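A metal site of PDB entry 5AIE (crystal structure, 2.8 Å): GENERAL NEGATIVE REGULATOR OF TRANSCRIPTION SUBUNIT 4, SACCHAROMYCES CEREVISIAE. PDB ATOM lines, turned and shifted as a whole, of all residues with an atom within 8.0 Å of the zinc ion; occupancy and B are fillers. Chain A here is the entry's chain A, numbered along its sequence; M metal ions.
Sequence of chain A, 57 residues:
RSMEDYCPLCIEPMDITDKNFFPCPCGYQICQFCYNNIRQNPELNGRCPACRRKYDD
The backbone NH (N) of Tyr 28 lies close to the side-chain sulfur (SG) of Cys 26. The side-chain sulfur (SG) of Cys 48 lies close to the backbone NH (N) of Ala 50, at 3.4 Å. The backbone NH (N) of Cys 48 sits at hydrogen-bond distance from the backbone carbonyl oxygen (O) of Arg 53.
The zinc ion is bound by SG of Cys 51, SG of Cys 26, SG of Cys 24 and SG of Cys 48.
Within 4 Å of the zinc ion: Cys 24, Cys 26, Cys 48 and Cys 51.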
ATOM      1  N   PRO A  23      -1.706   8.139  -5.128  1.00  0.00           N
ATOM      2  CA  PRO A  23      -2.396   8.109  -6.415  1.00  0.00           C
ATOM      3  C   PRO A  23      -3.875   7.735  -6.311  1.00  0.00           C
ATOM      4  O   PRO A  23      -4.658   8.068  -7.207  1.00  0.00           O
ATOM      5  CB  PRO A  23      -1.617   7.047  -7.203  1.00  0.00           C
ATOM      6  CG  PRO A  23      -1.031   6.175  -6.158  1.00  0.00           C
ATOM      7  CD  PRO A  23      -0.700   7.077  -5.011  1.00  0.00           C
ATOM      8  N   CYS A  24      -4.249   7.058  -5.234  1.00  0.00           N
ATOM      9  CA  CYS A  24      -5.629   6.643  -5.025  1.00  0.00           C
ATOM     10  C   CYS A  24      -6.098   7.034  -3.630  1.00  0.00           C
ATOM     11  O   CYS A  24      -5.344   6.914  -2.658  1.00  0.00           O
ATOM     12  CB  CYS A  24      -5.753   5.128  -5.228  1.00  0.00           C
ATOM     13  SG  CYS A  24      -7.447   4.512  -5.318  1.00  0.00           S
ATOM     14  N   PRO A  25      -7.349   7.519  -3.514  1.00  0.00           N
ATOM     15  CA  PRO A  25      -7.943   7.935  -2.238  1.00  0.00           C
ATOM     16  C   PRO A  25      -7.989   6.837  -1.179  1.00  0.00           C
ATOM     17  O   PRO A  25      -8.191   7.130   0.002  1.00  0.00           O
ATOM     18  CB  PRO A  25      -9.361   8.373  -2.629  1.00  0.00           C
ATOM     19  CG  PRO A  25      -9.592   7.811  -4.001  1.00  0.00           C
ATOM     20  CD  PRO A  25      -8.247   7.810  -4.649  1.00  0.00           C
ATOM     21  N   CYS A  26      -7.820   5.578  -1.595  1.00  0.00           N
ATOM     22  CA  CYS A  26      -7.880   4.458  -0.666  1.00  0.00           C
ATOM     23  C   CYS A  26      -6.643   4.405   0.237  1.00  0.00           C
ATOM     24  O   CYS A  26      -6.702   3.883   1.354  1.00  0.00           O
ATOM     25  CB  CYS A  26      -8.028   3.136  -1.426  1.00  0.00           C
ATOM     26  SG  CYS A  26      -6.575   2.651  -2.363  1.00  0.00           S
ATOM     27  N   GLY A  27      -5.530   4.935  -0.260  1.00  0.00           N
ATOM     28  CA  GLY A  27      -4.306   4.993   0.525  1.00  0.00           C
ATOM     29  C   GLY A  27      -3.249   3.983   0.125  1.00  0.00           C
ATOM     30  O   GLY A  27      -2.172   3.947   0.711  1.00  0.00           O
ATOM     31  N   TYR A  28      -3.558   3.164  -0.882  1.00  0.00           N
ATOM     32  CA  TYR A  28      -2.616   2.168  -1.367  1.00  0.00           C
ATOM     33  C   TYR A  28      -1.455   2.844  -2.095  1.00  0.00           C
ATOM     34  O   TYR A  28      -1.661   3.544  -3.083  1.00  0.00           O
ATOM     35  CB  TYR A  28      -3.322   1.163  -2.276  1.00  0.00           C
ATOM     36  CG  TYR A  28      -2.538  -0.105  -2.527  1.00  0.00           C
ATOM     37  CD1 TYR A  28      -2.334  -1.024  -1.509  1.00  0.00           C
ATOM     38  CD2 TYR A  28      -2.015  -0.384  -3.788  1.00  0.00           C
ATOM     39  CE1 TYR A  28      -1.615  -2.185  -1.733  1.00  0.00           C
ATOM     40  CE2 TYR A  28      -1.297  -1.545  -4.012  1.00  0.00           C
ATOM     41  CZ  TYR A  28      -1.105  -2.437  -2.984  1.00  0.00           C
ATOM     42  OH  TYR A  28      -0.393  -3.600  -3.201  1.00  0.00           O
ATOM     43  N   GLN A  29      -0.239   2.621  -1.604  1.00  0.00           N
ATOM     44  CA  GLN A  29       0.934   3.303  -2.155  1.00  0.00           C
ATOM     45  C   GLN A  29       1.826   2.381  -2.980  1.00  0.00           C
ATOM     46  O   GLN A  29       2.197   1.298  -2.546  1.00  0.00           O
ATOM     47  CB  GLN A  29       1.751   3.929  -1.022  1.00  0.00           C
ATOM     48  CG  GLN A  29       1.079   5.084  -0.317  1.00  0.00           C
ATOM     49  CD  GLN A  29       1.987   5.773   0.681  1.00  0.00           C
ATOM     50  OE1 GLN A  29       2.296   5.212   1.732  1.00  0.00           O
ATOM     51  NE2 GLN A  29       2.425   6.985   0.365  1.00  0.00           N
ATOM     52  N   ARG A  47      -5.604   0.788 -13.117  1.00  0.00           N
ATOM     53  CA  ARG A  47      -6.368   1.135 -11.916  1.00  0.00           C
ATOM     54  C   ARG A  47      -5.671   0.625 -10.654  1.00  0.00           C
ATOM     55  O   ARG A  47      -4.736  -0.175 -10.745  1.00  0.00           O
ATOM     56  CB  ARG A  47      -7.794   0.586 -12.008  1.00  0.00           C
ATOM     57  CG  ARG A  47      -7.891  -0.814 -12.593  1.00  0.00           C
ATOM     58  CD  ARG A  47      -9.334  -1.285 -12.677  1.00  0.00           C
ATOM     59  NE  ARG A  47     -10.197  -0.305 -13.335  1.00  0.00           N
ATOM     60  CZ  ARG A  47     -11.471  -0.522 -13.648  1.00  0.00           C
ATOM     61  NH1 ARG A  47     -12.030  -1.684 -13.370  1.00  0.00           N
ATOM     62  NH2 ARG A  47     -12.182   0.433 -14.245  1.00  0.00           N
ATOM     63  N   CYS A  48      -6.127   1.083  -9.503  1.00  0.00           N
ATOM     64  CA  CYS A  48      -5.501   0.732  -8.231  1.00  0.00           C
ATOM     65  C   CYS A  48      -5.603  -0.767  -7.928  1.00  0.00           C
ATOM     66  O   CYS A  48      -6.688  -1.350  -7.985  1.00  0.00           O
ATOM     67  CB  CYS A  48      -6.139   1.532  -7.089  1.00  0.00           C
ATOM     68  SG  CYS A  48      -5.470   1.144  -5.460  1.00  0.00           S
ATOM     69  N   PRO A  49      -4.459  -1.389  -7.603  1.00  0.00           N
ATOM     70  CA  PRO A  49      -4.387  -2.821  -7.290  1.00  0.00           C
ATOM     71  C   PRO A  49      -5.192  -3.215  -6.051  1.00  0.00           C
ATOM     72  O   PRO A  49      -5.362  -4.405  -5.804  1.00  0.00           O
ATOM     73  CB  PRO A  49      -2.883  -3.042  -7.035  1.00  0.00           C
ATOM     74  CG  PRO A  49      -2.213  -1.936  -7.764  1.00  0.00           C
ATOM     75  CD  PRO A  49      -3.134  -0.757  -7.634  1.00  0.00           C
ATOM     76  N   ALA A  50      -5.679  -2.242  -5.301  1.00  0.00           N
ATOM     77  CA  ALA A  50      -6.454  -2.513  -4.096  1.00  0.00           C
ATOM     78  C   ALA A  50      -7.959  -2.456  -4.359  1.00  0.00           C
ATOM     79  O   ALA A  50      -8.616  -3.483  -4.405  1.00  0.00           O
ATOM     80  CB  ALA A  50      -6.067  -1.542  -3.002  1.00  0.00           C
ATOM     81  N   CYS A  51      -8.485  -1.247  -4.525  1.00  0.00           N
ATOM     82  CA  CYS A  51      -9.926  -1.058  -4.637  1.00  0.00           C
ATOM     83  C   CYS A  51     -10.393  -0.902  -6.084  1.00  0.00           C
ATOM     84  O   CYS A  51     -11.547  -0.556  -6.333  1.00  0.00           O
ATOM     85  CB  CYS A  51     -10.361   0.157  -3.826  1.00  0.00           C
ATOM     86  SG  CYS A  51      -9.753   1.743  -4.446  1.00  0.00           S
ATOM     87  N   ARG A  52      -9.490  -1.152  -7.035  1.00  0.00           N
ATOM     88  CA  ARG A  52      -9.806  -1.130  -8.466  1.00  0.00           C
ATOM     89  C   ARG A  52     -10.363   0.207  -8.953  1.00  0.00           C
ATOM     90  O   ARG A  52     -11.034   0.268  -9.978  1.00  0.00           O
ATOM     91  CB  ARG A  52     -10.802  -2.242  -8.801  1.00  0.00           C
ATOM     92  CG  ARG A  52     -10.310  -3.638  -8.472  1.00  0.00           C
ATOM     93  CD  ARG A  52     -11.279  -4.697  -8.973  1.00  0.00           C
ATOM     94  NE  ARG A  52     -11.383  -4.690 -10.424  1.00  0.00           N
ATOM     95  CZ  ARG A  52     -10.595  -5.389 -11.238  1.00  0.00           C
ATOM     96  NH1 ARG A  52      -9.645  -6.162 -10.730  1.00  0.00           N
ATOM     97  NH2 ARG A  52     -10.756  -5.326 -12.546  1.00  0.00           N
ATOM     98  N   ARG A  53     -10.069   1.285  -8.215  1.00  0.00           N
ATOM     99  CA  ARG A  53     -10.532   2.602  -8.609  1.00  0.00           C
ATOM    100  C   ARG A  53      -9.626   3.157  -9.711  1.00  0.00           C
ATOM    101  O   ARG A  53      -8.405   3.079  -9.627  1.00  0.00           O
ATOM    102  CB  ARG A  53     -10.550   3.558  -7.402  1.00  0.00           C
ATOM    103  CG  ARG A  53     -11.539   4.707  -7.534  1.00  0.00           C
ATOM    104  CD  ARG A  53     -11.463   5.631  -6.321  1.00  0.00           C
ATOM    105  NE  ARG A  53     -11.902   4.976  -5.089  1.00  0.00           N
ATOM    106  CZ  ARG A  53     -12.980   5.327  -4.390  1.00  0.00           C
ATOM    107  NH1 ARG A  53     -13.745   6.326  -4.816  1.00  0.00           N
ATOM    108  NH2 ARG A  53     -13.294   4.679  -3.277  1.00  0.00           N
ATOM    109  N   LYS A  54     -10.243   3.704 -10.754  1.00  0.00           N
ATOM    110  CA  LYS A  54      -9.495   4.211 -11.902  1.00  0.00           C
ATOM    111  C   LYS A  54      -8.704   5.472 -11.543  1.00  0.00           C
ATOM    112  O   LYS A  54      -9.185   6.348 -10.831  1.00  0.00           O
ATOM    113  CB  LYS A  54     -10.447   4.514 -13.068  1.00  0.00           C
ATOM    114  N   TYR A  55      -7.478   5.545 -12.058  1.00  0.00           N
ATOM    115  CA  TYR A  55      -6.617   6.698 -11.805  1.00  0.00           C
ATOM    116  C   TYR A  55      -7.065   7.915 -12.614  1.00  0.00           C
ATOM    117  O   TYR A  55      -7.747   7.788 -13.633  1.00  0.00           O
ATOM    118  CB  TYR A  55      -5.161   6.370 -12.132  1.00  0.00           C
ATOM    119  CG  TYR A  55      -4.522   5.404 -11.162  1.00  0.00           C
ATOM    120  CD1 TYR A  55      -4.245   5.776  -9.859  1.00  0.00           C
ATOM    121  CD2 TYR A  55      -4.185   4.108 -11.563  1.00  0.00           C
ATOM    122  CE1 TYR A  55      -3.655   4.891  -8.979  1.00  0.00           C
ATOM    123  CE2 TYR A  55      -3.596   3.222 -10.683  1.00  0.00           C
ATOM    124  CZ  TYR A  55      -3.325   3.625  -9.391  1.00  0.00           C
ATOM    125  OH  TYR A  55      -2.744   2.747  -8.503  1.00  0.00           O
HETATM  126 ZN    ZN M   1      -7.474   2.240  -4.511  1.00  0.00          ZN
